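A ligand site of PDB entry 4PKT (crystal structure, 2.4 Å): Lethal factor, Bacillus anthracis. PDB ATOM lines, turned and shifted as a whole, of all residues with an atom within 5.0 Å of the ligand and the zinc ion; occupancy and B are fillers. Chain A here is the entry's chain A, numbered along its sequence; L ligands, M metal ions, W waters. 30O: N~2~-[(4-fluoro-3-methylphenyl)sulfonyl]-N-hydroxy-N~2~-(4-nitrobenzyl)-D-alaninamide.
Within 4 Å of the zinc ion: His 425, His 429 and Glu 474. Along chain A the residues within 4 Å of the zinc ion span positions 425 to 474.
NE2 of His 429 is bound to the zinc ion, at 2.0 Å. The zinc ion is bound by OE1 of Glu 474, at 2.1 Å. A ring nitrogen (NE2) of His 425 is bound to the zinc ion (2.3 Å). O5 of the ligand is bound to the zinc ion, 2.3 Å away. O3 of the ligand binds the zinc ion (2.3 Å). The zinc ion has five donor atoms within binding distance.
Water W1 bridges the backbone NH (N) of Tyr 398 and a nitrogen (N4) of the ligand.
The backbone carbonyl oxygen (O) of Ser 66 lies close to an oxygen (O1) of the ligand (2.9 Å). OE2 of Glu 478 sits close to F16 of the ligand (3.3 Å). NE of Arg 481 sits close to F16 of the ligand (3.5 Å). CA of Asp 67 touches C23 of the ligand (3.4 Å). CB of Ser 394 touches O9 of the ligand (3.6 Å). CD1 of Leu 397 touches N4 of the ligand, at 3.9 Å. Gly 413 touches the ligand. Val 414 touches the ligand (CG1 to O4, 3.2 Å). CG of Leu 416 touches C12 of the ligand, 3.5 Å away. Of the 23 residues printed, 17 come within 4 Å of the ligand.
O3 of the ligand lies close to OH of Tyr 467 (3.0 Å). The side-chain carboxylate (OE1) of Glu 426 lies within hydrogen-bond range of a nitrogen (N4) of the ligand (3.4 Å). NZ of Lys 74 is in hydrogen-bond range of O1 of the ligand, at 2.6 Å. N of Gly 396 lies within hydrogen-bond range of O9 of the ligand, 3.2 Å away. N of Lys 395 is in hydrogen-bond range of O9 of the ligand (3.1 Å). A nitrogen (N4) of the ligand is in hydrogen-bond range of the backbone carbonyl oxygen (O) of Gly 396, at 2.8 Å.
The side-chain carboxylate (OE1) of Glu 478 is in salt-bridge range of the guanidinium group (NH2) of Arg 481 (2.7 Å). The side-chain carboxylate (OE2) of Glu 478 is in hydrogen-bond range of a ring nitrogen (ND1) of His 425 (3.1 Å). NZ of Lys 74 lies within hydrogen-bond range of O of Ser 66 (3.0 Å). The side-chain hydroxyl (OH) of Tyr 467 lies close to the side-chain carboxylate (OE2) of Glu 474, at 3.4 Å. OG of Ser 394 is in hydrogen-bond range of O of Gly 396 (3.0 Å). OE2 of Glu 426 sits at hydrogen-bond distance from N of Tyr 398. The side-chain carboxylate (OE1) of Glu 421 lies within salt-bridge range of the guanidinium group (NH1) of Arg 481 (3.9 Å). The backbone carbonyl oxygen (O) of Asp 64 lies within hydrogen-bond range of the side-chain amino group (NZ) of Lys 74, at 3.3 Å.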
ATOM      1  N   ASP A  64     -24.680   6.820   8.223  1.00  0.00           N
ATOM      2  CA  ASP A  64     -24.670   7.902   9.205  1.00  0.00           C
ATOM      3  C   ASP A  64     -23.768   7.608  10.401  1.00  0.00           C
ATOM      4  O   ASP A  64     -23.441   8.511  11.186  1.00  0.00           O
ATOM      5  CB  ASP A  64     -26.103   8.190   9.688  1.00  0.00           C
ATOM      6  CG  ASP A  64     -26.888   9.043   8.710  1.00  0.00           C
ATOM      7  OD1 ASP A  64     -26.262   9.639   7.810  1.00  0.00           O
ATOM      8  OD2 ASP A  64     -28.128   9.107   8.851  1.00  0.00           O
ATOM      9  N   SER A  66     -20.706   6.983  10.363  1.00  0.00           N
ATOM     10  CA  SER A  66     -19.326   7.248   9.978  1.00  0.00           C
ATOM     11  C   SER A  66     -18.837   8.518  10.649  1.00  0.00           C
ATOM     12  O   SER A  66     -19.553   9.514  10.696  1.00  0.00           O
ATOM     13  CB  SER A  66     -19.209   7.354   8.459  1.00  0.00           C
ATOM     14  OG  SER A  66     -17.863   7.596   8.066  1.00  0.00           O
ATOM     15  N   ASP A  67     -17.611   8.490  11.177  1.00  0.00           N
ATOM     16  CA  ASP A  67     -17.066   9.648  11.893  1.00  0.00           C
ATOM     17  C   ASP A  67     -16.033  10.424  11.081  1.00  0.00           C
ATOM     18  O   ASP A  67     -15.355  11.314  11.609  1.00  0.00           O
ATOM     19  CB  ASP A  67     -16.462   9.213  13.239  1.00  0.00           C
ATOM     20  CG  ASP A  67     -15.328   8.201  13.095  1.00  0.00           C
ATOM     21  OD1 ASP A  67     -15.154   7.625  11.993  1.00  0.00           O
ATOM     22  OD2 ASP A  67     -14.617   7.978  14.091  1.00  0.00           O
ATOM     23  N   LYS A  74     -22.228  12.041   3.233  1.00  0.00           N
ATOM     24  CA  LYS A  74     -23.134  11.004   3.722  1.00  0.00           C
ATOM     25  C   LYS A  74     -24.400  10.931   2.862  1.00  0.00           C
ATOM     26  O   LYS A  74     -24.912   9.851   2.607  1.00  0.00           O
ATOM     27  CB  LYS A  74     -23.492  11.256   5.196  1.00  0.00           C
ATOM     28  CG  LYS A  74     -22.360  10.945   6.176  1.00  0.00           C
ATOM     29  CD  LYS A  74     -22.713  11.305   7.613  1.00  0.00           C
ATOM     30  CE  LYS A  74     -21.628  10.826   8.576  1.00  0.00           C
ATOM     31  NZ  LYS A  74     -21.891  11.189   9.994  1.00  0.00           N
ATOM     32  N   SER A 394     -13.086  17.149  10.647  1.00  0.00           N
ATOM     33  CA  SER A 394     -14.043  17.050  11.729  1.00  0.00           C
ATOM     34  C   SER A 394     -13.953  18.306  12.571  1.00  0.00           C
ATOM     35  O   SER A 394     -13.199  19.224  12.251  1.00  0.00           O
ATOM     36  CB  SER A 394     -13.777  15.817  12.602  1.00  0.00           C
ATOM     37  OG  SER A 394     -12.484  15.877  13.183  1.00  0.00           O
ATOM     38  N   LYS A 395     -14.740  18.331  13.645  1.00  0.00           N
ATOM     39  CA  LYS A 395     -14.786  19.473  14.542  1.00  0.00           C
ATOM     40  C   LYS A 395     -13.462  19.631  15.253  1.00  0.00           C
ATOM     41  O   LYS A 395     -12.968  20.743  15.455  1.00  0.00           O
ATOM     42  CB  LYS A 395     -15.909  19.304  15.566  1.00  0.00           C
ATOM     43  CG  LYS A 395     -16.049  20.482  16.496  1.00  0.00           C
ATOM     44  CD  LYS A 395     -16.508  21.696  15.678  1.00  0.00           C
ATOM     45  CE  LYS A 395     -16.512  22.940  16.506  1.00  0.00           C
ATOM     46  NZ  LYS A 395     -16.986  24.108  15.735  1.00  0.00           N
ATOM     47  N   GLY A 396     -12.866  18.511  15.649  1.00  0.00           N
ATOM     48  CA  GLY A 396     -11.658  18.552  16.445  1.00  0.00           C
ATOM     49  C   GLY A 396     -10.848  17.274  16.300  1.00  0.00           C
ATOM     50  O   GLY A 396     -11.362  16.222  15.907  1.00  0.00           O
ATOM     51  N   LEU A 397      -9.572  17.368  16.639  1.00  0.00           N
ATOM     52  CA  LEU A 397      -8.669  16.248  16.455  1.00  0.00           C
ATOM     53  C   LEU A 397      -7.469  16.385  17.411  1.00  0.00           C
ATOM     54  O   LEU A 397      -7.031  17.491  17.749  1.00  0.00           O
ATOM     55  CB  LEU A 397      -8.198  16.203  14.980  1.00  0.00           C
ATOM     56  CG  LEU A 397      -7.931  14.855  14.288  1.00  0.00           C
ATOM     57  CD1 LEU A 397      -9.187  13.993  14.295  1.00  0.00           C
ATOM     58  CD2 LEU A 397      -7.456  15.091  12.837  1.00  0.00           C
ATOM     59  N   TYR A 398      -6.936  15.242  17.842  1.00  0.00           N
ATOM     60  CA  TYR A 398      -5.631  15.238  18.474  1.00  0.00           C
ATOM     61  C   TYR A 398      -4.707  14.392  17.624  1.00  0.00           C
ATOM     62  O   TYR A 398      -5.038  13.260  17.278  1.00  0.00           O
ATOM     63  CB  TYR A 398      -5.695  14.709  19.921  1.00  0.00           C
ATOM     64  CG  TYR A 398      -4.319  14.582  20.532  1.00  0.00           C
ATOM     65  CD1 TYR A 398      -3.583  15.713  20.869  1.00  0.00           C
ATOM     66  CD2 TYR A 398      -3.729  13.343  20.749  1.00  0.00           C
ATOM     67  CE1 TYR A 398      -2.326  15.628  21.389  1.00  0.00           C
ATOM     68  CE2 TYR A 398      -2.452  13.249  21.287  1.00  0.00           C
ATOM     69  CZ  TYR A 398      -1.756  14.396  21.597  1.00  0.00           C
ATOM     70  OH  TYR A 398      -0.482  14.347  22.129  1.00  0.00           O
ATOM     71  N   GLY A 413     -19.928  19.958  15.830  1.00  0.00           N
ATOM     72  CA  GLY A 413     -19.584  18.592  16.192  1.00  0.00           C
ATOM     73  C   GLY A 413     -20.823  17.772  16.436  1.00  0.00           C
ATOM     74  O   GLY A 413     -21.805  18.266  16.973  1.00  0.00           O
ATOM     75  N   VAL A 414     -20.782  16.507  16.047  1.00  0.00           N
ATOM     76  CA  VAL A 414     -21.911  15.612  16.267  1.00  0.00           C
ATOM     77  C   VAL A 414     -22.133  15.360  17.766  1.00  0.00           C
ATOM     78  O   VAL A 414     -21.277  14.791  18.452  1.00  0.00           O
ATOM     79  CB  VAL A 414     -21.746  14.274  15.535  1.00  0.00           C
ATOM     80  CG1 VAL A 414     -22.808  13.284  15.996  1.00  0.00           C
ATOM     81  CG2 VAL A 414     -21.815  14.482  14.028  1.00  0.00           C
ATOM     82  N   GLU A 415     -23.301  15.790  18.237  1.00  0.00           N
ATOM     83  CA  GLU A 415     -23.691  15.728  19.642  1.00  0.00           C
ATOM     84  C   GLU A 415     -22.723  16.480  20.548  1.00  0.00           C
ATOM     85  O   GLU A 415     -22.400  16.011  21.636  1.00  0.00           O
ATOM     86  CB  GLU A 415     -23.821  14.280  20.099  1.00  0.00           C
ATOM     87  CG  GLU A 415     -24.987  13.549  19.443  1.00  0.00           C
ATOM     88  CD  GLU A 415     -26.338  13.932  20.044  1.00  0.00           C
ATOM     89  OE1 GLU A 415     -26.722  13.352  21.089  1.00  0.00           O
ATOM     90  OE2 GLU A 415     -27.007  14.826  19.473  1.00  0.00           O
ATOM     91  N   LEU A 416     -22.280  17.655  20.104  1.00  0.00           N
ATOM     92  CA  LEU A 416     -21.466  18.550  20.921  1.00  0.00           C
ATOM     93  C   LEU A 416     -22.171  19.895  21.132  1.00  0.00           C
ATOM     94  O   LEU A 416     -22.554  20.535  20.167  1.00  0.00           O
ATOM     95  CB  LEU A 416     -20.102  18.789  20.283  1.00  0.00           C
ATOM     96  CG  LEU A 416     -18.852  18.076  20.763  1.00  0.00           C
ATOM     97  CD1 LEU A 416     -17.624  18.597  19.968  1.00  0.00           C
ATOM     98  CD2 LEU A 416     -18.655  18.249  22.255  1.00  0.00           C
ATOM     99  N   GLU A 421     -16.445  22.280  24.867  1.00  0.00           N
ATOM    100  CA  GLU A 421     -16.545  20.864  25.219  1.00  0.00           C
ATOM    101  C   GLU A 421     -15.686  20.016  24.282  1.00  0.00           C
ATOM    102  O   GLU A 421     -15.064  19.052  24.712  1.00  0.00           O
ATOM    103  CB  GLU A 421     -18.016  20.393  25.192  1.00  0.00           C
ATOM    104  CG  GLU A 421     -18.814  20.905  26.383  1.00  0.00           C
ATOM    105  CD  GLU A 421     -20.193  20.262  26.498  1.00  0.00           C
ATOM    106  OE1 GLU A 421     -20.706  19.742  25.475  1.00  0.00           O
ATOM    107  OE2 GLU A 421     -20.757  20.275  27.621  1.00  0.00           O
ATOM    108  N   GLY A 422     -15.645  20.403  23.008  1.00  0.00           N
ATOM    109  CA  GLY A 422     -14.859  19.692  22.024  1.00  0.00           C
ATOM    110  C   GLY A 422     -13.372  19.712  22.348  1.00  0.00           C
ATOM    111  O   GLY A 422     -12.682  18.701  22.233  1.00  0.00           O
ATOM    112  N   HIS A 425     -12.504  17.321  25.162  1.00  0.00           N
ATOM    113  CA  HIS A 425     -12.414  15.956  24.633  1.00  0.00           C
ATOM    114  C   HIS A 425     -11.040  15.730  24.001  1.00  0.00           C
ATOM    115  O   HIS A 425     -10.430  14.679  24.253  1.00  0.00           O
ATOM    116  CB  HIS A 425     -13.555  15.687  23.630  1.00  0.00           C
ATOM    117  CG  HIS A 425     -13.323  14.507  22.720  1.00  0.00           C
ATOM    118  ND1 HIS A 425     -14.064  13.356  22.779  1.00  0.00           N
ATOM    119  CD2 HIS A 425     -12.447  14.323  21.688  1.00  0.00           C
ATOM    120  CE1 HIS A 425     -13.651  12.503  21.858  1.00  0.00           C
ATOM    121  NE2 HIS A 425     -12.664  13.067  21.183  1.00  0.00           N
ATOM    122  N   GLU A 426     -10.557  16.683  23.194  1.00  0.00           N
ATOM    123  CA  GLU A 426      -9.264  16.463  22.522  1.00  0.00           C
ATOM    124  C   GLU A 426      -8.140  16.482  23.543  1.00  0.00           C
ATOM    125  O   GLU A 426      -7.189  15.720  23.421  1.00  0.00           O
ATOM    126  CB  GLU A 426      -8.990  17.525  21.444  1.00  0.00           C
ATOM    127  CG  GLU A 426     -10.127  17.801  20.473  1.00  0.00           C
ATOM    128  CD  GLU A 426     -10.543  16.592  19.655  1.00  0.00           C
ATOM    129  OE1 GLU A 426     -11.627  16.644  19.052  1.00  0.00           O
ATOM    130  OE2 GLU A 426      -9.788  15.593  19.597  1.00  0.00           O
ATOM    131  N   HIS A 429      -7.616  13.180  24.807  1.00  0.00           N
ATOM    132  CA  HIS A 429      -6.728  12.346  24.002  1.00  0.00           C
ATOM    133  C   HIS A 429      -5.256  12.595  24.354  1.00  0.00           C
ATOM    134  O   HIS A 429      -4.432  11.690  24.361  1.00  0.00           O
ATOM    135  CB  HIS A 429      -6.930  12.603  22.512  1.00  0.00           C
ATOM    136  CG  HIS A 429      -8.206  12.054  21.941  1.00  0.00           C
ATOM    137  ND1 HIS A 429      -8.532  10.705  21.996  1.00  0.00           N
ATOM    138  CD2 HIS A 429      -9.210  12.649  21.252  1.00  0.00           C
ATOM    139  CE1 HIS A 429      -9.684  10.516  21.381  1.00  0.00           C
ATOM    140  NE2 HIS A 429     -10.115  11.672  20.925  1.00  0.00           N
ATOM    141  N   TYR A 467     -21.081   7.514  20.770  1.00  0.00           N
ATOM    142  CA  TYR A 467     -19.780   7.610  20.114  1.00  0.00           C
ATOM    143  C   TYR A 467     -18.670   6.987  20.984  1.00  0.00           C
ATOM    144  O   TYR A 467     -17.663   6.515  20.466  1.00  0.00           O
ATOM    145  CB  TYR A 467     -19.472   9.067  19.757  1.00  0.00           C
ATOM    146  CG  TYR A 467     -18.140   9.241  19.075  1.00  0.00           C
ATOM    147  CD1 TYR A 467     -17.868   8.606  17.880  1.00  0.00           C
ATOM    148  CD2 TYR A 467     -17.143  10.022  19.641  1.00  0.00           C
ATOM    149  CE1 TYR A 467     -16.640   8.747  17.249  1.00  0.00           C
ATOM    150  CE2 TYR A 467     -15.922  10.180  19.027  1.00  0.00           C
ATOM    151  CZ  TYR A 467     -15.661   9.537  17.829  1.00  0.00           C
ATOM    152  OH  TYR A 467     -14.430   9.697  17.205  1.00  0.00           O
ATOM    153  N   GLU A 474     -11.514   6.802  22.146  1.00  0.00           N
ATOM    154  CA  GLU A 474     -12.639   7.717  22.161  1.00  0.00           C
ATOM    155  C   GLU A 474     -13.430   7.577  23.463  1.00  0.00           C
ATOM    156  O   GLU A 474     -13.868   8.578  24.033  1.00  0.00           O
ATOM    157  CB  GLU A 474     -13.569   7.500  20.967  1.00  0.00           C
ATOM    158  CG  GLU A 474     -12.918   7.609  19.579  1.00  0.00           C
ATOM    159  CD  GLU A 474     -12.211   8.933  19.316  1.00  0.00           C
ATOM    160  OE1 GLU A 474     -12.480   9.946  19.986  1.00  0.00           O
ATOM    161  OE2 GLU A 474     -11.347   8.961  18.421  1.00  0.00           O
ATOM    162  N   ALA A 477     -11.747   9.524  25.999  1.00  0.00           N
ATOM    163  CA  ALA A 477     -11.844  10.960  25.717  1.00  0.00           C
ATOM    164  C   ALA A 477     -13.241  11.463  26.031  1.00  0.00           C
ATOM    165  O   ALA A 477     -13.402  12.563  26.553  1.00  0.00           O
ATOM    166  CB  ALA A 477     -11.459  11.280  24.221  1.00  0.00           C
ATOM    167  N   GLU A 478     -14.249  10.665  25.703  1.00  0.00           N
ATOM    168  CA  GLU A 478     -15.614  11.034  26.077  1.00  0.00           C
ATOM    169  C   GLU A 478     -15.787  11.020  27.607  1.00  0.00           C
ATOM    170  O   GLU A 478     -16.335  11.965  28.177  1.00  0.00           O
ATOM    171  CB  GLU A 478     -16.627  10.110  25.407  1.00  0.00           C
ATOM    172  CG  GLU A 478     -16.825  10.402  23.908  1.00  0.00           C
ATOM    173  CD  GLU A 478     -17.577  11.714  23.652  1.00  0.00           C
ATOM    174  OE1 GLU A 478     -18.802  11.673  23.354  1.00  0.00           O
ATOM    175  OE2 GLU A 478     -16.950  12.797  23.750  1.00  0.00           O
ATOM    176  N   ARG A 481     -14.189  14.008  29.024  1.00  0.00           N
ATOM    177  CA  ARG A 481     -14.941  15.209  28.718  1.00  0.00           C
ATOM    178  C   ARG A 481     -16.159  15.305  29.644  1.00  0.00           C
ATOM    179  O   ARG A 481     -16.347  16.315  30.314  1.00  0.00           O
ATOM    180  CB  ARG A 481     -15.379  15.243  27.244  1.00  0.00           C
ATOM    181  CG  ARG A 481     -16.526  16.222  26.996  1.00  0.00           C
ATOM    182  CD  ARG A 481     -17.026  16.240  25.568  1.00  0.00           C
ATOM    183  NE  ARG A 481     -17.765  15.036  25.195  1.00  0.00           N
ATOM    184  CZ  ARG A 481     -19.097  14.911  25.279  1.00  0.00           C
ATOM    185  NH1 ARG A 481     -19.844  15.904  25.749  1.00  0.00           N
ATOM    186  NH2 ARG A 481     -19.673  13.785  24.882  1.00  0.00           N
HETATM  187  C21 30O L   1     -19.455  11.368  15.795  1.00  0.00           C
HETATM  188  C20 30O L   1     -18.287  11.721  16.456  1.00  0.00           C
HETATM  189  C22 30O L   1     -19.561  11.558  14.419  1.00  0.00           C
HETATM  190  C23 30O L   1     -18.486  12.114  13.721  1.00  0.00           C
HETATM  191  C24 30O L   1     -17.297  12.467  14.372  1.00  0.00           C
HETATM  192  C19 30O L   1     -17.213  12.268  15.754  1.00  0.00           C
HETATM  193  C18 30O L   1     -15.978  12.615  16.552  1.00  0.00           C
HETATM  194  N6  30O L   1     -15.283  13.865  16.263  1.00  0.00           N
HETATM  195  C1  30O L   1     -13.849  13.596  15.967  1.00  0.00           C
HETATM  196  C28 30O L   1     -13.715  12.475  14.940  1.00  0.00           C
HETATM  197  C2  30O L   1     -12.960  13.221  17.156  1.00  0.00           C
HETATM  198  N4  30O L   1     -11.781  13.819  17.236  1.00  0.00           N
HETATM  199  O5  30O L   1     -10.989  13.620  18.369  1.00  0.00           O
HETATM  200  O3  30O L   1     -13.271  12.382  18.015  1.00  0.00           O
HETATM  201  S7  30O L   1     -15.962  15.263  16.430  1.00  0.00           S
HETATM  202  O8  30O L   1     -17.277  15.387  15.828  1.00  0.00           O
HETATM  203  O9  30O L   1     -15.087  16.296  15.939  1.00  0.00           O
HETATM  204  C10 30O L   1     -16.066  15.357  18.019  1.00  0.00           C
HETATM  205  C15 30O L   1     -14.959  15.821  18.730  1.00  0.00           C
HETATM  206  C14 30O L   1     -15.028  15.872  20.114  1.00  0.00           C
HETATM  207  C13 30O L   1     -16.176  15.449  20.774  1.00  0.00           C
HETATM  208  F16 30O L   1     -16.212  15.532  22.116  1.00  0.00           F
HETATM  209  C12 30O L   1     -17.285  14.969  20.079  1.00  0.00           C
HETATM  210  C11 30O L   1     -17.227  14.913  18.682  1.00  0.00           C
HETATM  211  C17 30O L   1     -18.517  14.507  20.798  1.00  0.00           C
HETATM  212  N1  30O L   1     -20.762  11.193  13.775  1.00  0.00           N
HETATM  213  O1  30O L   1     -20.920  11.372  12.395  1.00  0.00           O
HETATM  214  O4  30O L   1     -21.813  10.649  14.520  1.00  0.00           O
HETATM  215 ZN    ZN M   1     -11.655  11.807  19.605  1.00  0.00          ZN
HETATM  216  O   HOH W   1      -8.558  12.601  17.373  1.00  0.00           O
